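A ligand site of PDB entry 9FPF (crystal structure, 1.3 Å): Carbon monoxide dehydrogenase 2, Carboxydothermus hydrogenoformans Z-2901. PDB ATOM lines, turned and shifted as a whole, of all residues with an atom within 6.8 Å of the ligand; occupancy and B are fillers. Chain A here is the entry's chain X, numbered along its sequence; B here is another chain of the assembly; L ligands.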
ATOM      1  N   CYS A  47     -26.917 -30.964  12.735  1.00  0.00           N
ATOM      2  CA  CYS A  47     -26.977 -30.188  13.959  1.00  0.00           C
ATOM      3  C   CYS A  47     -25.942 -29.078  13.885  1.00  0.00           C
ATOM      4  O   CYS A  47     -24.833 -29.279  13.369  1.00  0.00           O
ATOM      5  CB  CYS A  47     -26.707 -31.044  15.204  1.00  0.00           C
ATOM      6  SG  CYS A  47     -26.728 -30.061  16.732  1.00  0.00           S
ATOM      7  N   CYS A  48     -26.322 -27.894  14.366  1.00  0.00           N
ATOM      8  CA  CYS A  48     -25.428 -26.741  14.377  1.00  0.00           C
ATOM      9  C   CYS A  48     -25.556 -26.037  15.721  1.00  0.00           C
ATOM     10  O   CYS A  48     -26.666 -25.736  16.174  1.00  0.00           O
ATOM     11  CB  CYS A  48     -25.768 -25.793  13.228  1.00  0.00           C
ATOM     12  SG  CYS A  48     -24.695 -24.309  13.190  1.00  0.00           S
ATOM     13  N   ARG A  49     -24.407 -25.732  16.335  1.00  0.00           N
ATOM     14  CA  ARG A  49     -24.302 -24.937  17.556  1.00  0.00           C
ATOM     15  C   ARG A  49     -23.366 -23.751  17.358  1.00  0.00           C
ATOM     16  O   ARG A  49     -22.678 -23.326  18.291  1.00  0.00           O
ATOM     17  CB  ARG A  49     -23.868 -25.810  18.725  1.00  0.00           C
ATOM     18  CG  ARG A  49     -24.860 -26.918  19.007  1.00  0.00           C
ATOM     19  CD  ARG A  49     -24.273 -27.952  19.980  1.00  0.00           C
ATOM     20  NE  ARG A  49     -23.886 -27.316  21.226  1.00  0.00           N
ATOM     21  CZ  ARG A  49     -23.003 -27.790  22.093  1.00  0.00           C
ATOM     22  NH1 ARG A  49     -22.378 -28.944  21.881  1.00  0.00           N
ATOM     23  NH2 ARG A  49     -22.731 -27.081  23.190  1.00  0.00           N
ATOM     24  N   HIS A  50     -23.307 -23.199  16.142  1.00  0.00           N
ATOM     25  CA  HIS A  50     -22.355 -22.133  15.848  1.00  0.00           C
ATOM     26  C   HIS A  50     -22.820 -20.752  16.329  1.00  0.00           C
ATOM     27  O   HIS A  50     -22.031 -19.802  16.188  1.00  0.00           O
ATOM     28  CB  HIS A  50     -22.009 -22.110  14.358  1.00  0.00           C
ATOM     29  CG  HIS A  50     -21.205 -23.302  13.910  1.00  0.00           C
ATOM     30  ND1 HIS A  50     -20.502 -23.329  12.729  1.00  0.00           N
ATOM     31  CD2 HIS A  50     -21.025 -24.526  14.471  1.00  0.00           C
ATOM     32  CE1 HIS A  50     -19.939 -24.516  12.570  1.00  0.00           C
ATOM     33  NE2 HIS A  50     -20.239 -25.265  13.621  1.00  0.00           N
ATOM     34  N   CYS A  51     -23.997 -20.616  16.935  1.00  0.00           N
ATOM     35  CA  CYS A  51     -24.354 -19.363  17.596  1.00  0.00           C
ATOM     36  C   CYS A  51     -25.345 -19.631  18.719  1.00  0.00           C
ATOM     37  O   CYS A  51     -25.864 -20.744  18.873  1.00  0.00           O
ATOM     38  CB  CYS A  51     -24.883 -18.314  16.607  1.00  0.00           C
ATOM     39  SG  CYS A  51     -26.662 -18.441  16.194  1.00  0.00           S
ATOM     40  N   LEU A  52     -25.631 -18.591  19.514  1.00  0.00           N
ATOM     41  CA  LEU A  52     -26.473 -18.738  20.694  1.00  0.00           C
ATOM     42  C   LEU A  52     -27.975 -18.702  20.375  1.00  0.00           C
ATOM     43  O   LEU A  52     -28.789 -18.768  21.306  1.00  0.00           O
ATOM     44  CB  LEU A  52     -26.102 -17.722  21.786  1.00  0.00           C
ATOM     45  CG  LEU A  52     -24.659 -17.743  22.262  1.00  0.00           C
ATOM     46  CD1 LEU A  52     -24.488 -16.673  23.332  1.00  0.00           C
ATOM     47  CD2 LEU A  52     -24.299 -19.089  22.805  1.00  0.00           C
ATOM     48  N   GLN A  53     -28.363 -18.646  19.105  1.00  0.00           N
ATOM     49  CA  GLN A  53     -29.738 -18.936  18.726  1.00  0.00           C
ATOM     50  C   GLN A  53     -29.988 -20.429  18.667  1.00  0.00           C
ATOM     51  O   GLN A  53     -31.150 -20.848  18.724  1.00  0.00           O
ATOM     52  CB  GLN A  53     -30.091 -18.297  17.381  1.00  0.00           C
ATOM     53  CG  GLN A  53     -30.124 -16.795  17.491  1.00  0.00           C
ATOM     54  CD  GLN A  53     -30.468 -16.081  16.204  1.00  0.00           C
ATOM     55  OE1 GLN A  53     -30.290 -16.592  15.087  1.00  0.00           O
ATOM     56  NE2 GLN A  53     -30.965 -14.903  16.329  1.00  0.00           N
ATOM     57  N   GLY A  54     -28.923 -21.227  18.553  1.00  0.00           N
ATOM     58  CA  GLY A  54     -29.065 -22.665  18.531  1.00  0.00           C
ATOM     59  C   GLY A  54     -29.301 -23.238  19.914  1.00  0.00           C
ATOM     60  O   GLY A  54     -29.480 -22.530  20.905  1.00  0.00           O
ATOM     61  N   PRO A  55     -29.287 -24.561  20.006  1.00  0.00           N
ATOM     62  CA  PRO A  55     -28.929 -25.503  18.942  1.00  0.00           C
ATOM     63  C   PRO A  55     -30.015 -25.609  17.881  1.00  0.00           C
ATOM     64  O   PRO A  55     -31.222 -25.601  18.162  1.00  0.00           O
ATOM     65  CB  PRO A  55     -28.753 -26.834  19.700  1.00  0.00           C
ATOM     66  CG  PRO A  55     -29.656 -26.682  20.920  1.00  0.00           C
ATOM     67  CD  PRO A  55     -29.583 -25.227  21.286  1.00  0.00           C
ATOM     68  N   CYS A  56     -29.562 -25.738  16.651  1.00  0.00           N
ATOM     69  CA  CYS A  56     -30.430 -25.996  15.524  1.00  0.00           C
ATOM     70  C   CYS A  56     -30.212 -27.409  15.017  1.00  0.00           C
ATOM     71  O   CYS A  56     -29.110 -27.960  15.112  1.00  0.00           O
ATOM     72  CB  CYS A  56     -30.129 -25.016  14.384  1.00  0.00           C
ATOM     73  SG  CYS A  56     -30.658 -23.307  14.731  1.00  0.00           S
ATOM     74  N   ARG A  57     -31.265 -27.976  14.442  1.00  0.00           N
ATOM     75  CA  ARG A  57     -31.192 -29.295  13.854  1.00  0.00           C
ATOM     76  C   ARG A  57     -32.111 -29.309  12.646  1.00  0.00           C
ATOM     77  O   ARG A  57     -32.991 -28.444  12.496  1.00  0.00           O
ATOM     78  CB  ARG A  57     -31.619 -30.366  14.866  1.00  0.00           C
ATOM     79  CG  ARG A  57     -33.117 -30.377  15.156  1.00  0.00           C
ATOM     80  CD  ARG A  57     -33.466 -31.059  16.466  1.00  0.00           C
ATOM     81  NE  ARG A  57     -34.912 -31.090  16.652  1.00  0.00           N
ATOM     82  CZ  ARG A  57     -35.643 -30.025  16.980  1.00  0.00           C
ATOM     83  NH1 ARG A  57     -35.077 -28.896  17.379  1.00  0.00           N
ATOM     84  NH2 ARG A  57     -36.966 -30.109  16.908  1.00  0.00           N
ATOM     85  N   VAL A  67     -34.621 -26.287   8.138  1.00  0.00           N
ATOM     86  CA  VAL A  67     -33.584 -25.295   7.876  1.00  0.00           C
ATOM     87  C   VAL A  67     -33.211 -24.690   9.221  1.00  0.00           C
ATOM     88  O   VAL A  67     -34.019 -24.664  10.145  1.00  0.00           O
ATOM     89  CB  VAL A  67     -34.123 -24.232   6.876  1.00  0.00           C
ATOM     90  CG1 VAL A  67     -35.369 -23.558   7.414  1.00  0.00           C
ATOM     91  CG2 VAL A  67     -33.105 -23.215   6.553  1.00  0.00           C
ATOM     92  N   GLY A  68     -31.955 -24.230   9.337  1.00  0.00           N
ATOM     93  CA  GLY A  68     -31.519 -23.571  10.548  1.00  0.00           C
ATOM     94  C   GLY A  68     -32.201 -22.229  10.759  1.00  0.00           C
ATOM     95  O   GLY A  68     -32.752 -21.641   9.830  1.00  0.00           O
ATOM     96  N   ILE A  69     -32.120 -21.727  11.986  1.00  0.00           N
ATOM     97  CA  ILE A  69     -32.834 -20.495  12.329  1.00  0.00           C
ATOM     98  C   ILE A  69     -32.366 -19.312  11.477  1.00  0.00           C
ATOM     99  O   ILE A  69     -33.193 -18.498  11.031  1.00  0.00           O
ATOM    100  CB  ILE A  69     -32.743 -20.208  13.849  1.00  0.00           C
ATOM    101  CG1 ILE A  69     -33.601 -21.212  14.619  1.00  0.00           C
ATOM    102  CG2 ILE A  69     -33.160 -18.759  14.171  1.00  0.00           C
ATOM    103  CD1 ILE A  69     -33.378 -21.198  16.115  1.00  0.00           C
ATOM    104  N   CYS A  70     -31.062 -19.200  11.195  1.00  0.00           N
ATOM    105  CA  CYS A  70     -30.546 -18.116  10.363  1.00  0.00           C
ATOM    106  C   CYS A  70     -30.782 -18.338   8.872  1.00  0.00           C
ATOM    107  O   CYS A  70     -30.424 -17.472   8.058  1.00  0.00           O
ATOM    108  CB  CYS A  70     -29.047 -17.995  10.599  1.00  0.00           C
ATOM    109  SG  CYS A  70     -28.122 -19.483  10.130  1.00  0.00           S
ATOM    110  N   GLY A  71     -31.325 -19.482   8.488  1.00  0.00           N
ATOM    111  CA  GLY A  71     -31.467 -19.866   7.097  1.00  0.00           C
ATOM    112  C   GLY A  71     -30.449 -20.883   6.585  1.00  0.00           C
ATOM    113  O   GLY A  71     -30.518 -21.252   5.410  1.00  0.00           O
ATOM    114  N   ALA A  72     -29.522 -21.340   7.432  1.00  0.00           N
ATOM    115  CA  ALA A  72     -28.505 -22.309   7.010  1.00  0.00           C
ATOM    116  C   ALA A  72     -29.173 -23.611   6.576  1.00  0.00           C
ATOM    117  O   ALA A  72     -29.932 -24.227   7.329  1.00  0.00           O
ATOM    118  CB  ALA A  72     -27.551 -22.545   8.187  1.00  0.00           C
ATOM    119  N   ILE A  77     -24.864 -26.571   6.773  1.00  0.00           N
ATOM    120  CA  ILE A  77     -24.574 -27.074   8.118  1.00  0.00           C
ATOM    121  C   ILE A  77     -23.602 -28.249   8.063  1.00  0.00           C
ATOM    122  O   ILE A  77     -22.611 -28.302   8.800  1.00  0.00           O
ATOM    123  CB  ILE A  77     -25.899 -27.430   8.826  1.00  0.00           C
ATOM    124  CG1 ILE A  77     -26.644 -26.136   9.179  1.00  0.00           C
ATOM    125  CG2 ILE A  77     -25.670 -28.310  10.046  1.00  0.00           C
ATOM    126  CD1 ILE A  77     -28.043 -26.338   9.796  1.00  0.00           C
ATOM    127  N   ARG A  80     -20.062 -26.997   7.002  1.00  0.00           N
ATOM    128  CA  ARG A  80     -19.391 -26.213   8.038  1.00  0.00           C
ATOM    129  C   ARG A  80     -18.858 -27.099   9.156  1.00  0.00           C
ATOM    130  O   ARG A  80     -17.733 -26.904   9.633  1.00  0.00           O
ATOM    131  CB  ARG A  80     -20.372 -25.166   8.621  1.00  0.00           C
ATOM    132  CG  ARG A  80     -20.735 -24.068   7.608  1.00  0.00           C
ATOM    133  CD  ARG A  80     -21.412 -22.844   8.242  1.00  0.00           C
ATOM    134  NE  ARG A  80     -22.581 -23.179   9.046  1.00  0.00           N
ATOM    135  CZ  ARG A  80     -23.462 -22.286   9.471  1.00  0.00           C
ATOM    136  NH1 ARG A  80     -23.354 -21.010   9.167  1.00  0.00           N
ATOM    137  NH2 ARG A  80     -24.488 -22.692  10.225  1.00  0.00           N
ATOM    138  N   THR A 197     -16.836 -20.497   8.680  1.00  0.00           N
ATOM    139  CA  THR A 197     -17.862 -21.389   9.185  1.00  0.00           C
ATOM    140  C   THR A 197     -18.658 -20.797  10.350  1.00  0.00           C
ATOM    141  O   THR A 197     -19.640 -21.416  10.791  1.00  0.00           O
ATOM    142  CB  THR A 197     -17.272 -22.731   9.633  1.00  0.00           C
ATOM    143  OG1 THR A 197     -16.286 -22.495  10.630  1.00  0.00           O
ATOM    144  CG2 THR A 197     -16.678 -23.501   8.447  1.00  0.00           C
ATOM    145  N   SER A 198     -18.264 -19.627  10.844  1.00  0.00           N
ATOM    146  CA  SER A 198     -19.017 -18.937  11.889  1.00  0.00           C
ATOM    147  C   SER A 198     -20.296 -18.373  11.300  1.00  0.00           C
ATOM    148  O   SER A 198     -20.501 -18.346  10.080  1.00  0.00           O
ATOM    149  CB  SER A 198     -18.134 -17.881  12.570  1.00  0.00           C
ATOM    150  OG  SER A 198     -17.973 -16.698  11.800  1.00  0.00           O
ATOM    151  N   MET A 199     -21.204 -17.979  12.168  1.00  0.00           N
ATOM    152  CA  MET A 199     -22.541 -17.605  11.716  1.00  0.00           C
ATOM    153  C   MET A 199     -22.485 -16.445  10.732  1.00  0.00           C
ATOM    154  O   MET A 199     -21.758 -15.455  10.919  1.00  0.00           O
ATOM    155  CB  MET A 199     -23.444 -17.272  12.912  1.00  0.00           C
ATOM    156  CG  MET A 199     -24.888 -16.878  12.542  1.00  0.00           C
ATOM    157  SD  MET A 199     -25.028 -15.152  12.020  1.00  0.00           S
ATOM    158  CE  MET A 199     -26.410 -15.210  10.877  1.00  0.00           C
ATOM    159  N   GLY A 200     -23.294 -16.559   9.680  1.00  0.00           N
ATOM    160  CA  GLY A 200     -23.505 -15.451   8.771  1.00  0.00           C
ATOM    161  C   GLY A 200     -22.334 -15.182   7.839  1.00  0.00           C
ATOM    162  O   GLY A 200     -22.187 -14.041   7.366  1.00  0.00           O
ATOM    163  N   MET B  35     -38.249 -24.672  15.075  1.00  0.00           N
ATOM    164  CA  MET B  35     -37.168 -25.371  15.738  1.00  0.00           C
ATOM    165  C   MET B  35     -37.524 -25.795  17.153  1.00  0.00           C
ATOM    166  O   MET B  35     -36.775 -26.586  17.748  1.00  0.00           O
ATOM    167  CB  MET B  35     -35.951 -24.447  15.783  1.00  0.00           C
ATOM    168  CG  MET B  35     -34.612 -25.172  16.048  1.00  0.00           C
ATOM    169  SD  MET B  35     -34.216 -26.383  14.753  1.00  0.00           S
ATOM    170  CE  MET B  35     -33.754 -25.408  13.374  1.00  0.00           C
ATOM    171  N   GLN B  38     -36.092 -26.823  21.298  1.00  0.00           N
ATOM    172  CA  GLN B  38     -34.702 -27.025  20.953  1.00  0.00           C
ATOM    173  C   GLN B  38     -34.077 -28.064  21.885  1.00  0.00           C
ATOM    174  O   GLN B  38     -34.557 -28.329  22.994  1.00  0.00           O
ATOM    175  CB  GLN B  38     -33.942 -25.697  21.000  1.00  0.00           C
ATOM    176  CG  GLN B  38     -34.400 -24.710  19.930  1.00  0.00           C
ATOM    177  CD  GLN B  38     -33.692 -23.375  20.015  1.00  0.00           C
ATOM    178  OE1 GLN B  38     -34.066 -22.515  20.809  1.00  0.00           O
ATOM    179  NE2 GLN B  38     -32.661 -23.214  19.209  1.00  0.00           N
ATOM    180  N   PRO B 336     -28.208 -16.308   5.872  1.00  0.00           N
ATOM    181  CA  PRO B 336     -28.205 -16.764   4.483  1.00  0.00           C
ATOM    182  C   PRO B 336     -29.586 -16.846   3.854  1.00  0.00           C
ATOM    183  O   PRO B 336     -29.686 -16.932   2.621  1.00  0.00           O
ATOM    184  CB  PRO B 336     -27.490 -18.120   4.541  1.00  0.00           C
ATOM    185  CG  PRO B 336     -27.614 -18.563   5.955  1.00  0.00           C
ATOM    186  CD  PRO B 336     -27.601 -17.305   6.781  1.00  0.00           C
ATOM    187  N   MET B 560     -25.621 -13.255  20.508  1.00  0.00           N
ATOM    188  CA  MET B 560     -25.832 -14.331  19.538  1.00  0.00           C
ATOM    189  C   MET B 560     -24.537 -14.937  18.980  1.00  0.00           C
ATOM    190  O   MET B 560     -24.306 -16.159  19.078  1.00  0.00           O
ATOM    191  CB  MET B 560     -26.707 -13.820  18.390  1.00  0.00           C
ATOM    192  CG  MET B 560     -27.010 -14.798  17.279  1.00  0.00           C
ATOM    193  SD  MET B 560     -25.872 -14.785  15.879  1.00  0.00           S
ATOM    194  CE  MET B 560     -26.043 -13.098  15.254  1.00  0.00           C
HETATM  195 FE1  LIG L   1     -26.182 -22.535  13.468  1.00  0.00          FE
HETATM  196 FE2  LIG L   1     -26.851 -20.258  14.755  1.00  0.00          FE
HETATM  197 FE3  LIG L   1     -28.736 -22.096  14.154  1.00  0.00          FE
HETATM  198 FE4  LIG L   1     -27.614 -20.643  12.115  1.00  0.00          FE
HETATM  199  S1  LIG L   1     -28.960 -19.857  13.848  1.00  0.00           S
HETATM  200  S2  LIG L   1     -27.998 -22.864  12.074  1.00  0.00           S
HETATM  201  S3  LIG L   1     -25.436 -20.471  12.922  1.00  0.00           S
HETATM  202  S4  LIG L   1     -26.953 -22.356  15.615  1.00  0.00           S
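The guanidinium group (NH2) of Arg 80 sits close to a sulfur (S3) of the ligand (3.6 Å).
SG of Cys 48 binds FE1 of the ligand, 2.3 Å away.
S4 of the ligand lies close to N of Gly 54.
An iron atom (FE2) of the ligand is bound by the side-chain sulfur (SG) of Cys 51.
The backbone NH (N) of Cys 51 lies close to a sulfur (S4) of the ligand (3.7 Å).
A sulfur (S1) of the ligand lies close to the backbone NH (N) of Cys 70, at 3.4 Å.
N of His 50 lies close to S4 of the ligand (3.8 Å).
FE4 of the ligand is bound by SG of Cys 70, at 2.4 Å.
The side-chain sulfur (SG) of Cys 56 binds an iron atom (FE3) of the ligand (2.3 Å).
The side-chain amide oxygen of Gln 53 sits close to a sulfur (S1) of the ligand, 3.7 Å away.
The side-chain amide nitrogen of Gln 38 of chain B sits at hydrogen-bond distance from the backbone carbonyl oxygen of Gln 53.
SG of Cys 70 sits close to N of Ala 72 (3.6 Å).
The side-chain sulfur of Cys 47 sits close to the backbone carbonyl oxygen of Cys 56 (3.6 Å).
The backbone carbonyl oxygen (O) of Cys 56 sits at hydrogen-bond distance from the backbone NH (N) of Cys 48, at 2.9 Å.
SG of Cys 48 sits close to NH2 of Arg 80 (3.4 Å).
The side-chain sulfur (SD) of Met 560 of chain B sits close to the side-chain sulfur (SG) of Cys 51.
N of Gln 53 sits close to SG of Cys 51 (3.4 Å).
The side-chain sulfur (SG) of Cys 56 lies close to the backbone NH (N) of Ile 69 (3.5 Å).
CA of Gly 68 touches S2 of the ligand (3.9 Å).
Ile 69 touches the ligand.
CB of Ala 72 touches S2 of the ligand (3.9 Å).
Met 199 touches the ligand.
Within 4 Å of the ligand: Cys 48, His 50, Cys 51, Gln 53, Gly 54, Cys 56, Gly 68, Ile 69, Cys 70, Ala 72, Arg 80 and Met 199.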
